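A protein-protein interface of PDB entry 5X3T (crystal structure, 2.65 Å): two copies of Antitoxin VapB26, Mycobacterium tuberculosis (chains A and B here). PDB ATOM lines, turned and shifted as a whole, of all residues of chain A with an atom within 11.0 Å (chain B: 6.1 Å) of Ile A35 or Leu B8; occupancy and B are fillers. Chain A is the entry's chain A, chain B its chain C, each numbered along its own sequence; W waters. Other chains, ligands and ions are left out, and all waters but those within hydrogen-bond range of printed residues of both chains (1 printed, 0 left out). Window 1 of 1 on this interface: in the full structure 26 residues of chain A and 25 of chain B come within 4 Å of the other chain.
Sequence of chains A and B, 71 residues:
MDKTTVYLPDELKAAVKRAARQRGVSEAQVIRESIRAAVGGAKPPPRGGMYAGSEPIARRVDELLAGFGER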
ATOM      1  N   MET A   1     -27.945   6.900 -25.419  1.00  0.00           N
ATOM      2  CA  MET A   1     -26.780   6.989 -24.554  1.00  0.00           C
ATOM      3  C   MET A   1     -25.606   7.579 -25.318  1.00  0.00           C
ATOM      4  O   MET A   1     -25.048   6.932 -26.203  1.00  0.00           O
ATOM      5  CB  MET A   1     -26.409   5.610 -24.000  1.00  0.00           C
ATOM      6  CG  MET A   1     -25.484   5.665 -22.799  1.00  0.00           C
ATOM      7  SD  MET A   1     -26.562   6.119 -21.251  1.00  0.00           S
ATOM      8  CE  MET A   1     -25.469   5.382 -19.834  1.00  0.00           C
ATOM      9  N   ASP A   2     -25.242   8.812 -24.982  1.00  0.00           N
ATOM     10  CA  ASP A   2     -24.126   9.475 -25.640  1.00  0.00           C
ATOM     11  C   ASP A   2     -22.832   9.173 -24.914  1.00  0.00           C
ATOM     12  O   ASP A   2     -22.773   9.201 -23.685  1.00  0.00           O
ATOM     13  CB  ASP A   2     -24.344  10.992 -25.714  1.00  0.00           C
ATOM     14  CG  ASP A   2     -25.425  11.380 -26.709  1.00  0.00           C
ATOM     15  OD1 ASP A   2     -25.779  10.536 -27.555  1.00  0.00           O
ATOM     16  OD2 ASP A   2     -25.924  12.524 -26.646  1.00  0.00           O
ATOM     17  N   LYS A   3     -21.790   8.896 -25.685  1.00  0.00           N
ATOM     18  CA  LYS A   3     -20.487   8.625 -25.115  1.00  0.00           C
ATOM     19  C   LYS A   3     -19.711   9.928 -24.977  1.00  0.00           C
ATOM     20  O   LYS A   3     -19.350  10.558 -25.970  1.00  0.00           O
ATOM     21  CB  LYS A   3     -19.730   7.619 -25.984  1.00  0.00           C
ATOM     22  CG  LYS A   3     -18.236   7.596 -25.740  1.00  0.00           C
ATOM     23  CD  LYS A   3     -17.628   6.226 -26.029  1.00  0.00           C
ATOM     24  CE  LYS A   3     -18.360   5.463 -27.126  1.00  0.00           C
ATOM     25  NZ  LYS A   3     -18.442   4.011 -26.796  1.00  0.00           N
ATOM     26  N   THR A   4     -19.453  10.317 -23.732  1.00  0.00           N
ATOM     27  CA  THR A   4     -18.763  11.567 -23.431  1.00  0.00           C
ATOM     28  C   THR A   4     -17.355  11.314 -22.900  1.00  0.00           C
ATOM     29  O   THR A   4     -17.126  10.376 -22.137  1.00  0.00           O
ATOM     30  CB  THR A   4     -19.551  12.401 -22.399  1.00  0.00           C
ATOM     31  OG1 THR A   4     -20.863  12.666 -22.905  1.00  0.00           O
ATOM     32  CG2 THR A   4     -18.852  13.729 -22.103  1.00  0.00           C
ATOM     33  N   THR A   5     -16.415  12.154 -23.314  1.00  0.00           N
ATOM     34  CA  THR A   5     -15.043  12.066 -22.842  1.00  0.00           C
ATOM     35  C   THR A   5     -14.630  13.365 -22.164  1.00  0.00           C
ATOM     36  O   THR A   5     -14.684  14.436 -22.769  1.00  0.00           O
ATOM     37  CB  THR A   5     -14.077  11.764 -23.990  1.00  0.00           C
ATOM     38  OG1 THR A   5     -14.316  12.684 -25.062  1.00  0.00           O
ATOM     39  CG2 THR A   5     -14.287  10.346 -24.497  1.00  0.00           C
ATOM     40  N   VAL A   6     -14.229  13.273 -20.904  1.00  0.00           N
ATOM     41  CA  VAL A   6     -13.805  14.456 -20.170  1.00  0.00           C
ATOM     42  C   VAL A   6     -12.424  14.264 -19.573  1.00  0.00           C
ATOM     43  O   VAL A   6     -12.064  13.161 -19.163  1.00  0.00           O
ATOM     44  CB  VAL A   6     -14.793  14.813 -19.044  1.00  0.00           C
ATOM     45  CG1 VAL A   6     -16.146  15.141 -19.630  1.00  0.00           C
ATOM     46  CG2 VAL A   6     -14.907  13.671 -18.038  1.00  0.00           C
ATOM     47  N   TYR A   7     -11.638  15.332 -19.536  1.00  0.00           N
ATOM     48  CA  TYR A   7     -10.404  15.279 -18.772  1.00  0.00           C
ATOM     49  C   TYR A   7     -10.718  15.517 -17.305  1.00  0.00           C
ATOM     50  O   TYR A   7     -11.366  16.499 -16.944  1.00  0.00           O
ATOM     51  CB  TYR A   7      -9.372  16.296 -19.258  1.00  0.00           C
ATOM     52  CG  TYR A   7      -8.008  16.057 -18.641  1.00  0.00           C
ATOM     53  CD1 TYR A   7      -7.104  15.176 -19.220  1.00  0.00           C
ATOM     54  CD2 TYR A   7      -7.644  16.678 -17.450  1.00  0.00           C
ATOM     55  CE1 TYR A   7      -5.864  14.941 -18.646  1.00  0.00           C
ATOM     56  CE2 TYR A   7      -6.410  16.449 -16.868  1.00  0.00           C
ATOM     57  CZ  TYR A   7      -5.524  15.581 -17.468  1.00  0.00           C
ATOM     58  OH  TYR A   7      -4.296  15.357 -16.884  1.00  0.00           O
ATOM     59  N   LEU A   8     -10.286  14.583 -16.468  1.00  0.00           N
ATOM     60  CA  LEU A   8     -10.385  14.722 -15.023  1.00  0.00           C
ATOM     61  C   LEU A   8      -8.970  14.787 -14.469  1.00  0.00           C
ATOM     62  O   LEU A   8      -8.185  13.863 -14.688  1.00  0.00           O
ATOM     63  CB  LEU A   8     -11.158  13.553 -14.411  1.00  0.00           C
ATOM     64  CG  LEU A   8     -12.622  13.413 -14.837  1.00  0.00           C
ATOM     65  CD1 LEU A   8     -13.268  12.191 -14.197  1.00  0.00           C
ATOM     66  CD2 LEU A   8     -13.401  14.675 -14.497  1.00  0.00           C
ATOM     67  N   LEU A  12      -8.889  14.780  -8.818  1.00  0.00           N
ATOM     68  CA  LEU A  12     -10.318  14.539  -8.826  1.00  0.00           C
ATOM     69  C   LEU A  12     -10.625  13.069  -9.050  1.00  0.00           C
ATOM     70  O   LEU A  12     -11.583  12.530  -8.499  1.00  0.00           O
ATOM     71  CB  LEU A  12     -10.964  15.384  -9.922  1.00  0.00           C
ATOM     72  CG  LEU A  12     -12.418  15.827  -9.810  1.00  0.00           C
ATOM     73  CD1 LEU A  12     -12.580  16.638  -8.547  1.00  0.00           C
ATOM     74  CD2 LEU A  12     -12.735  16.672 -11.024  1.00  0.00           C
ATOM     75  N   VAL A  16     -12.582  10.675  -6.534  1.00  0.00           N
ATOM     76  CA  VAL A  16     -13.638   9.778  -6.993  1.00  0.00           C
ATOM     77  C   VAL A  16     -13.349   8.338  -6.606  1.00  0.00           C
ATOM     78  O   VAL A  16     -14.231   7.641  -6.114  1.00  0.00           O
ATOM     79  CB  VAL A  16     -13.818   9.853  -8.523  1.00  0.00           C
ATOM     80  CG1 VAL A  16     -14.682   8.705  -9.025  1.00  0.00           C
ATOM     81  CG2 VAL A  16     -14.418  11.178  -8.915  1.00  0.00           C
ATOM     82  N   GLU A  27     -16.659   3.590  -9.984  1.00  0.00           N
ATOM     83  CA  GLU A  27     -16.307   5.004 -10.121  1.00  0.00           C
ATOM     84  C   GLU A  27     -17.316   5.702 -11.039  1.00  0.00           C
ATOM     85  O   GLU A  27     -17.684   6.872 -10.836  1.00  0.00           O
ATOM     86  CB  GLU A  27     -14.877   5.145 -10.659  1.00  0.00           C
ATOM     87  CG  GLU A  27     -13.802   4.711  -9.663  1.00  0.00           C
ATOM     88  CD  GLU A  27     -12.393   4.918 -10.184  1.00  0.00           C
ATOM     89  OE1 GLU A  27     -12.247   5.447 -11.305  1.00  0.00           O
ATOM     90  OE2 GLU A  27     -11.432   4.555  -9.470  1.00  0.00           O
ATOM     91  N   ALA A  28     -17.769   4.950 -12.038  1.00  0.00           N
ATOM     92  CA  ALA A  28     -18.791   5.395 -12.974  1.00  0.00           C
ATOM     93  C   ALA A  28     -20.050   5.880 -12.260  1.00  0.00           C
ATOM     94  O   ALA A  28     -20.571   6.957 -12.560  1.00  0.00           O
ATOM     95  CB  ALA A  28     -19.136   4.273 -13.936  1.00  0.00           C
ATOM     96  N   GLN A  29     -20.531   5.075 -11.315  1.00  0.00           N
ATOM     97  CA  GLN A  29     -21.750   5.390 -10.579  1.00  0.00           C
ATOM     98  C   GLN A  29     -21.594   6.663  -9.751  1.00  0.00           C
ATOM     99  O   GLN A  29     -22.500   7.502  -9.717  1.00  0.00           O
ATOM    100  CB  GLN A  29     -22.156   4.221  -9.678  1.00  0.00           C
ATOM    101  CG  GLN A  29     -23.512   4.414  -9.009  1.00  0.00           C
ATOM    102  CD  GLN A  29     -23.753   3.461  -7.852  1.00  0.00           C
ATOM    103  OE1 GLN A  29     -23.388   2.288  -7.910  1.00  0.00           O
ATOM    104  NE2 GLN A  29     -24.387   3.963  -6.796  1.00  0.00           N
ATOM    105  N   VAL A  30     -20.449   6.800  -9.086  1.00  0.00           N
ATOM    106  CA  VAL A  30     -20.140   8.002  -8.319  1.00  0.00           C
ATOM    107  C   VAL A  30     -20.209   9.231  -9.219  1.00  0.00           C
ATOM    108  O   VAL A  30     -20.832  10.240  -8.867  1.00  0.00           O
ATOM    109  CB  VAL A  30     -18.740   7.925  -7.670  1.00  0.00           C
ATOM    110  CG1 VAL A  30     -18.395   9.239  -6.979  1.00  0.00           C
ATOM    111  CG2 VAL A  30     -18.660   6.757  -6.695  1.00  0.00           C
ATOM    112  N   ILE A  31     -19.578   9.132 -10.386  1.00  0.00           N
ATOM    113  CA  ILE A  31     -19.574  10.240 -11.338  1.00  0.00           C
ATOM    114  C   ILE A  31     -20.993  10.603 -11.807  1.00  0.00           C
ATOM    115  O   ILE A  31     -21.388  11.780 -11.767  1.00  0.00           O
ATOM    116  CB  ILE A  31     -18.681   9.917 -12.558  1.00  0.00           C
ATOM    117  CG1 ILE A  31     -17.206   9.896 -12.143  1.00  0.00           C
ATOM    118  CG2 ILE A  31     -18.901  10.928 -13.666  1.00  0.00           C
ATOM    119  CD1 ILE A  31     -16.278   9.375 -13.215  1.00  0.00           C
ATOM    120  N   ARG A  32     -21.762   9.600 -12.232  1.00  0.00           N
ATOM    121  CA  ARG A  32     -23.137   9.829 -12.683  1.00  0.00           C
ATOM    122  C   ARG A  32     -23.985  10.494 -11.606  1.00  0.00           C
ATOM    123  O   ARG A  32     -24.689  11.472 -11.869  1.00  0.00           O
ATOM    124  CB  ARG A  32     -23.793   8.513 -13.119  1.00  0.00           C
ATOM    125  CG  ARG A  32     -25.224   8.680 -13.621  1.00  0.00           C
ATOM    126  CD  ARG A  32     -25.727   7.445 -14.369  1.00  0.00           C
ATOM    127  NE  ARG A  32     -24.772   6.967 -15.366  1.00  0.00           N
ATOM    128  CZ  ARG A  32     -24.913   5.839 -16.056  1.00  0.00           C
ATOM    129  NH1 ARG A  32     -25.979   5.072 -15.872  1.00  0.00           N
ATOM    130  NH2 ARG A  32     -23.992   5.479 -16.940  1.00  0.00           N
ATOM    131  N   GLU A  33     -23.907   9.957 -10.393  1.00  0.00           N
ATOM    132  CA  GLU A  33     -24.655  10.503  -9.272  1.00  0.00           C
ATOM    133  C   GLU A  33     -24.255  11.945  -8.972  1.00  0.00           C
ATOM    134  O   GLU A  33     -25.119  12.782  -8.709  1.00  0.00           O
ATOM    135  CB  GLU A  33     -24.469   9.639  -8.024  1.00  0.00           C
ATOM    136  CG  GLU A  33     -25.157   8.282  -8.103  1.00  0.00           C
ATOM    137  CD  GLU A  33     -24.904   7.428  -6.874  1.00  0.00           C
ATOM    138  OE1 GLU A  33     -24.289   7.937  -5.914  1.00  0.00           O
ATOM    139  OE2 GLU A  33     -25.320   6.248  -6.869  1.00  0.00           O
ATOM    140  N   SER A  34     -22.956  12.236  -9.015  1.00  0.00           N
ATOM    141  CA  SER A  34     -22.473  13.596  -8.776  1.00  0.00           C
ATOM    142  C   SER A  34     -23.077  14.564  -9.787  1.00  0.00           C
ATOM    143  O   SER A  34     -23.668  15.595  -9.424  1.00  0.00           O
ATOM    144  CB  SER A  34     -20.944  13.648  -8.848  1.00  0.00           C
ATOM    145  OG  SER A  34     -20.351  12.715  -7.953  1.00  0.00           O
ATOM    146  N   ILE A  35     -22.940  14.202 -11.059  1.00  0.00           N
ATOM    147  CA  ILE A  35     -23.471  15.014 -12.151  1.00  0.00           C
ATOM    148  C   ILE A  35     -24.977  15.255 -12.021  1.00  0.00           C
ATOM    149  O   ILE A  35     -25.429  16.397 -12.110  1.00  0.00           O
ATOM    150  CB  ILE A  35     -23.196  14.361 -13.513  1.00  0.00           C
ATOM    151  CG1 ILE A  35     -21.687  14.251 -13.766  1.00  0.00           C
ATOM    152  CG2 ILE A  35     -23.843  15.159 -14.622  1.00  0.00           C
ATOM    153  CD1 ILE A  35     -21.337  13.408 -14.978  1.00  0.00           C
ATOM    154  N   ARG A  36     -25.748  14.184 -11.827  1.00  0.00           N
ATOM    155  CA  ARG A  36     -27.193  14.313 -11.619  1.00  0.00           C
ATOM    156  C   ARG A  36     -27.517  15.224 -10.450  1.00  0.00           C
ATOM    157  O   ARG A  36     -28.446  16.025 -10.515  1.00  0.00           O
ATOM    158  CB  ARG A  36     -27.847  12.942 -11.393  1.00  0.00           C
ATOM    159  CG  ARG A  36     -29.320  13.046 -11.007  1.00  0.00           C
ATOM    160  CD  ARG A  36     -30.090  11.774 -11.304  1.00  0.00           C
ATOM    161  NE  ARG A  36     -31.463  11.847 -10.810  1.00  0.00           N
ATOM    162  CZ  ARG A  36     -32.545  11.647 -11.557  1.00  0.00           C
ATOM    163  NH1 ARG A  36     -32.425  11.373 -12.848  1.00  0.00           N
ATOM    164  NH2 ARG A  36     -33.752  11.730 -11.012  1.00  0.00           N
ATOM    165  N   ALA A  37     -26.748  15.087  -9.381  1.00  0.00           N
ATOM    166  CA  ALA A  37     -26.931  15.923  -8.208  1.00  0.00           C
ATOM    167  C   ALA A  37     -26.723  17.395  -8.540  1.00  0.00           C
ATOM    168  O   ALA A  37     -27.439  18.252  -8.028  1.00  0.00           O
ATOM    169  CB  ALA A  37     -25.993  15.497  -7.099  1.00  0.00           C
ATOM    170  N   ALA A  38     -25.739  17.699  -9.385  1.00  0.00           N
ATOM    171  CA  ALA A  38     -25.481  19.104  -9.727  1.00  0.00           C
ATOM    172  C   ALA A  38     -26.457  19.702 -10.752  1.00  0.00           C
ATOM    173  O   ALA A  38     -27.022  20.769 -10.516  1.00  0.00           O
ATOM    174  CB  ALA A  38     -24.054  19.268 -10.220  1.00  0.00           C
ATOM    175  N   VAL A  39     -26.639  19.031 -11.889  1.00  0.00           N
ATOM    176  CA  VAL A  39     -27.459  19.587 -12.974  1.00  0.00           C
ATOM    177  C   VAL A  39     -28.895  19.068 -13.060  1.00  0.00           C
ATOM    178  O   VAL A  39     -29.672  19.548 -13.889  1.00  0.00           O
ATOM    179  CB  VAL A  39     -26.823  19.332 -14.342  1.00  0.00           C
ATOM    180  CG1 VAL A  39     -25.440  19.945 -14.399  1.00  0.00           C
ATOM    181  CG2 VAL A  39     -26.756  17.845 -14.625  1.00  0.00           C
ATOM    182  N   GLY A  40     -29.246  18.091 -12.227  1.00  0.00           N
ATOM    183  CA  GLY A  40     -30.568  17.491 -12.279  1.00  0.00           C
ATOM    184  C   GLY A  40     -30.780  16.541 -13.445  1.00  0.00           C
ATOM    185  O   GLY A  40     -29.870  16.271 -14.231  1.00  0.00           O
ATOM    186  N   GLY A  41     -32.004  16.037 -13.543  1.00  0.00           N
ATOM    187  CA  GLY A  41     -32.427  15.123 -14.586  1.00  0.00           C
ATOM    188  C   GLY A  41     -33.154  15.879 -15.678  1.00  0.00           C
ATOM    189  O   GLY A  41     -32.752  16.981 -16.057  1.00  0.00           O
ATOM    190  N   ALA A  42     -34.203  15.257 -16.208  1.00  0.00           N
ATOM    191  CA  ALA A  42     -35.088  15.899 -17.175  1.00  0.00           C
ATOM    192  C   ALA A  42     -35.528  17.252 -16.644  1.00  0.00           C
ATOM    193  O   ALA A  42     -35.753  17.411 -15.445  1.00  0.00           O
ATOM    194  CB  ALA A  42     -36.302  15.025 -17.457  1.00  0.00           C
ATOM    195  N   VAL B   6     -17.243   8.760 -20.001  1.00  0.00           N
ATOM    196  CA  VAL B   6     -18.450   8.868 -19.199  1.00  0.00           C
ATOM    197  C   VAL B   6     -19.678   8.637 -20.066  1.00  0.00           C
ATOM    198  O   VAL B   6     -19.898   9.357 -21.040  1.00  0.00           O
ATOM    199  CB  VAL B   6     -18.572  10.247 -18.522  1.00  0.00           C
ATOM    200  CG1 VAL B   6     -19.888  10.345 -17.767  1.00  0.00           C
ATOM    201  CG2 VAL B   6     -17.386  10.510 -17.605  1.00  0.00           C
ATOM    202  N   TYR B   7     -20.471   7.628 -19.722  1.00  0.00           N
ATOM    203  CA  TYR B   7     -21.717   7.391 -20.437  1.00  0.00           C
ATOM    204  C   TYR B   7     -22.865   8.100 -19.727  1.00  0.00           C
ATOM    205  O   TYR B   7     -23.152   7.843 -18.557  1.00  0.00           O
ATOM    206  CB  TYR B   7     -21.992   5.892 -20.580  1.00  0.00           C
ATOM    207  CG  TYR B   7     -21.047   5.186 -21.536  1.00  0.00           C
ATOM    208  CD1 TYR B   7     -21.259   5.221 -22.911  1.00  0.00           C
ATOM    209  CD2 TYR B   7     -19.947   4.483 -21.064  1.00  0.00           C
ATOM    210  CE1 TYR B   7     -20.397   4.580 -23.789  1.00  0.00           C
ATOM    211  CE2 TYR B   7     -19.080   3.836 -21.935  1.00  0.00           C
ATOM    212  CZ  TYR B   7     -19.310   3.888 -23.296  1.00  0.00           C
ATOM    213  OH  TYR B   7     -18.450   3.248 -24.164  1.00  0.00           O
ATOM    214  N   LEU B   8     -23.480   9.032 -20.445  1.00  0.00           N
ATOM    215  CA  LEU B   8     -24.585   9.821 -19.923  1.00  0.00           C
ATOM    216  C   LEU B   8     -25.907   9.411 -20.560  1.00  0.00           C
ATOM    217  O   LEU B   8     -26.009   9.349 -21.786  1.00  0.00           O
ATOM    218  CB  LEU B   8     -24.334  11.310 -20.161  1.00  0.00           C
ATOM    219  CG  LEU B   8     -23.067  11.875 -19.519  1.00  0.00           C
ATOM    220  CD1 LEU B   8     -22.797  13.303 -19.980  1.00  0.00           C
ATOM    221  CD2 LEU B   8     -23.175  11.809 -18.002  1.00  0.00           C
ATOM    222  N   PRO B   9     -26.918   9.099 -19.734  1.00  0.00           N
ATOM    223  CA  PRO B   9     -28.272   9.000 -20.289  1.00  0.00           C
ATOM    224  C   PRO B   9     -28.668  10.330 -20.920  1.00  0.00           C
ATOM    225  O   PRO B   9     -28.145  11.368 -20.518  1.00  0.00           O
ATOM    226  CB  PRO B   9     -29.139   8.661 -19.072  1.00  0.00           C
ATOM    227  CG  PRO B   9     -28.182   8.142 -18.038  1.00  0.00           C
ATOM    228  CD  PRO B   9     -26.890   8.855 -18.281  1.00  0.00           C
ATOM    229  N   ASP B  10     -29.562  10.299 -21.903  1.00  0.00           N
ATOM    230  CA  ASP B  10     -29.887  11.501 -22.670  1.00  0.00           C
ATOM    231  C   ASP B  10     -30.499  12.597 -21.806  1.00  0.00           C
ATOM    232  O   ASP B  10     -30.303  13.787 -22.064  1.00  0.00           O
ATOM    233  CB  ASP B  10     -30.826  11.146 -23.824  1.00  0.00           C
ATOM    234  CG  ASP B  10     -30.157  10.261 -24.852  1.00  0.00           C
ATOM    235  OD1 ASP B  10     -29.006  10.569 -25.227  1.00  0.00           O
ATOM    236  OD2 ASP B  10     -30.771   9.263 -25.285  1.00  0.00           O
ATOM    237  N   GLU B  11     -31.232  12.182 -20.780  1.00  0.00           N
ATOM    238  CA  GLU B  11     -31.792  13.099 -19.799  1.00  0.00           C
ATOM    239  C   GLU B  11     -30.675  13.955 -19.205  1.00  0.00           C
ATOM    240  O   GLU B  11     -30.718  15.201 -19.200  1.00  0.00           O
ATOM    241  CB  GLU B  11     -32.500  12.310 -18.699  1.00  0.00           C
ATOM    242  CG  GLU B  11     -33.898  12.775 -18.409  1.00  0.00           C
ATOM    243  CD  GLU B  11     -34.547  12.011 -17.273  1.00  0.00           C
ATOM    244  OE1 GLU B  11     -34.265  12.346 -16.104  1.00  0.00           O
ATOM    245  OE2 GLU B  11     -35.346  11.092 -17.552  1.00  0.00           O
ATOM    246  N   LEU B  12     -29.649  13.251 -18.744  1.00  0.00           N
ATOM    247  CA  LEU B  12     -28.528  13.840 -18.041  1.00  0.00           C
ATOM    248  C   LEU B  12     -27.621  14.634 -18.981  1.00  0.00           C
ATOM    249  O   LEU B  12     -27.095  15.686 -18.607  1.00  0.00           O
ATOM    250  CB  LEU B  12     -27.743  12.729 -17.344  1.00  0.00           C
ATOM    251  CG  LEU B  12     -26.779  13.150 -16.248  1.00  0.00           C
ATOM    252  CD1 LEU B  12     -27.575  13.842 -15.165  1.00  0.00           C
ATOM    253  CD2 LEU B  12     -26.035  11.945 -15.683  1.00  0.00           C
ATOM    254  N   LYS B  13     -27.439  14.120 -20.196  1.00  0.00           N
ATOM    255  CA  LYS B  13     -26.645  14.802 -21.214  1.00  0.00           C
ATOM    256  C   LYS B  13     -27.274  16.156 -21.530  1.00  0.00           C
ATOM    257  O   LYS B  13     -26.587  17.186 -21.589  1.00  0.00           O
ATOM    258  CB  LYS B  13     -26.544  13.955 -22.482  1.00  0.00           C
ATOM    259  CG  LYS B  13     -25.656  14.552 -23.563  1.00  0.00           C
ATOM    260  CD  LYS B  13     -24.223  14.700 -23.070  1.00  0.00           C
ATOM    261  CE  LYS B  13     -23.280  15.131 -24.183  1.00  0.00           C
ATOM    262  NZ  LYS B  13     -21.896  15.325 -23.669  1.00  0.00           N
ATOM    263  N   VAL B  16     -26.704  18.563 -18.659  1.00  0.00           N
ATOM    264  CA  VAL B  16     -25.343  19.102 -18.659  1.00  0.00           C
ATOM    265  C   VAL B  16     -25.192  20.196 -19.714  1.00  0.00           C
ATOM    266  O   VAL B  16     -24.690  21.290 -19.430  1.00  0.00           O
ATOM    267  CB  VAL B  16     -24.295  17.997 -18.901  1.00  0.00           C
ATOM    268  CG1 VAL B  16     -22.943  18.600 -19.238  1.00  0.00           C
ATOM    269  CG2 VAL B  16     -24.202  17.084 -17.683  1.00  0.00           C
ATOM    270  N   VAL B  30     -18.652  21.857 -16.382  1.00  0.00           N
ATOM    271  CA  VAL B  30     -19.844  21.538 -15.601  1.00  0.00           C
ATOM    272  C   VAL B  30     -19.682  20.179 -14.932  1.00  0.00           C
ATOM    273  O   VAL B  30     -19.941  20.024 -13.732  1.00  0.00           O
ATOM    274  CB  VAL B  30     -21.117  21.525 -16.470  1.00  0.00           C
ATOM    275  CG1 VAL B  30     -22.256  20.818 -15.748  1.00  0.00           C
ATOM    276  CG2 VAL B  30     -21.513  22.939 -16.860  1.00  0.00           C
ATOM    277  N   ILE B  31     -19.241  19.198 -15.717  1.00  0.00           N
ATOM    278  CA  ILE B  31     -19.014  17.856 -15.190  1.00  0.00           C
ATOM    279  C   ILE B  31     -17.970  17.842 -14.069  1.00  0.00           C
ATOM    280  O   ILE B  31     -18.221  17.305 -12.974  1.00  0.00           O
ATOM    281  CB  ILE B  31     -18.587  16.890 -16.311  1.00  0.00           C
ATOM    282  CG1 ILE B  31     -19.764  16.637 -17.260  1.00  0.00           C
ATOM    283  CG2 ILE B  31     -18.085  15.581 -15.723  1.00  0.00           C
ATOM    284  CD1 ILE B  31     -19.394  15.923 -18.535  1.00  0.00           C
ATOM    285  N   SER B  34     -19.297  19.428 -10.930  1.00  0.00           N
ATOM    286  CA  SER B  34     -20.263  18.519 -10.320  1.00  0.00           C
ATOM    287  C   SER B  34     -19.528  17.530  -9.428  1.00  0.00           C
ATOM    288  O   SER B  34     -19.816  17.383  -8.223  1.00  0.00           O
ATOM    289  CB  SER B  34     -21.058  17.767 -11.391  1.00  0.00           C
ATOM    290  OG  SER B  34     -21.757  18.658 -12.245  1.00  0.00           O
ATOM    291  N   ILE B  35     -18.555  16.863 -10.041  1.00  0.00           N
ATOM    292  CA  ILE B  35     -17.770  15.853  -9.346  1.00  0.00           C
ATOM    293  C   ILE B  35     -17.024  16.419  -8.140  1.00  0.00           C
ATOM    294  O   ILE B  35     -16.999  15.797  -7.082  1.00  0.00           O
ATOM    295  CB  ILE B  35     -16.774  15.186 -10.298  1.00  0.00           C
ATOM    296  CG1 ILE B  35     -17.541  14.437 -11.393  1.00  0.00           C
ATOM    297  CG2 ILE B  35     -15.856  14.256  -9.544  1.00  0.00           C
ATOM    298  CD1 ILE B  35     -16.674  13.933 -12.513  1.00  0.00           C
HETATM  299  O   HOH W   1     -22.378  17.218  -7.443  1.00  0.00           O
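The backbone NH (N) of Leu B8 is in hydrogen-bond range of the backbone carbonyl oxygen (O) of Asp A2 (3.3 Å). The side-chain hydroxyl (OH) of Tyr B7 is in hydrogen-bond range of the side-chain amino group (NZ) of Lys A3, at 2.7 Å. The backbone carbonyl oxygen (O) of Thr A4 is in hydrogen-bond range of the backbone NH (N) of Val B6, 2.7 Å away. The side-chain amino group (NZ) of Lys B13 sits at hydrogen-bond distance from the side-chain hydroxyl (OG1) of Thr A4 (3.0 Å). NH2 of Arg A32 sits at hydrogen-bond distance from O of Tyr B7 (3.0 Å). The side-chain carboxylate (OE1) of Glu B11 lies within salt-bridge range of the guanidinium group (NH1) of Arg A36 (3.9 Å). The backbone NH of Ala A42 is in hydrogen-bond range of the side-chain carboxylate of Glu B11, at 2.9 Å. O of Leu B8 lies close to SD of Met A1 (3.3 Å). The backbone nitrogen of Pro B9 sits close to the side-chain sulfur of Met A1 (3.4 Å).
O of Val A30 is in hydrogen-bond range of OG of Ser A34 (2.7 Å). The backbone carbonyl oxygen (O) of Val B30 sits at hydrogen-bond distance from the side-chain hydroxyl (OG) of Ser B34 (2.7 Å).
CE of Met A1 touches CB of Tyr B7 (3.6 Å). Val B6 touches Asp A2 (O to O, 3.9 Å). OD1 of Asp B10 touches OD2 of Asp A2 (3.9 Å). Thr A4 touches Leu B8. Val A6 touches Ile B31. Leu B12 touches Ile A35. Ile A35 touches Val B16 (CG2 to CG2, 3.6 Å). CG1 of Val A39 touches CG1 of Val B30, at 3.6 Å. Gly A40 touches Leu B12 (O to CD1, 3.5 Å). Gly A41 touches Glu B11.
Thr A5 touches none of the printed residues of chain B. Of the printed residues of chain B, Leu A8 touches Ile B35 (3.9 Å). Printed residues of chain B within 4 Å of Ile A35: Leu B8 (3.9 Å), Leu B12 (3.9 Å), Val B16 (3.6 Å), Ile B31 (3.98 Å) and Ser B34 (3.7 Å). Printed residues of chain B within 4 Å of Ala A38: Ser B34 (3.1 Å). Of chain A, only Met A1, Asp A2, Thr A4 and Ile A35 come within 4 Å of Leu B8. Of chain A, only Met A1 (3.4 Å) comes within 4 Å of Pro B9. Asp B10 touches two residues of chain A. The nearest residue of chain A that does not touch Leu B8 is Arg A32 (5.0 Å). The nearest printed residue of chain B that does not touch Met A1 is Val B6 (6.6 Å).
Hydrophobic or aromatic side chains of chain A within 4 Å of the printed part of chain B: Met A1, Val A6, Leu A8, Leu A12, Val A16, Ile A31, Ile A35, Ala A38, Val A39 and Ala A42. Among the printed residues, 35 pairs touch across the chains. Among the printed residues, Asp or Glu carboxylates within 4 Å of a Lys or Arg side-chain nitrogen of the other chain: Arg A36 with Glu B11 (3.9 Å).
Val A6 touches Ile B31, but with the chains exchanged Ile A31 does not touch Val B6 (4.2 Å). Leu A12 touches Ile B35, and with the chains exchanged Ile A35 touches Leu B12. Val A16 touches Ile B35, and with the chains exchanged Ile A35 touches Val B16. Ser A34 touches Ile B35, and with the chains exchanged Ile A35 touches Ser B34. 9 positions are printed for both chains. Of the 35 pairs that touch across the chains among the printed residues, 11 have their exchanged pair printed and touching as well.
Water W1 bridges the backbone carbonyl oxygen of Ser B34 and the backbone carbonyl oxygen of Ser A34.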
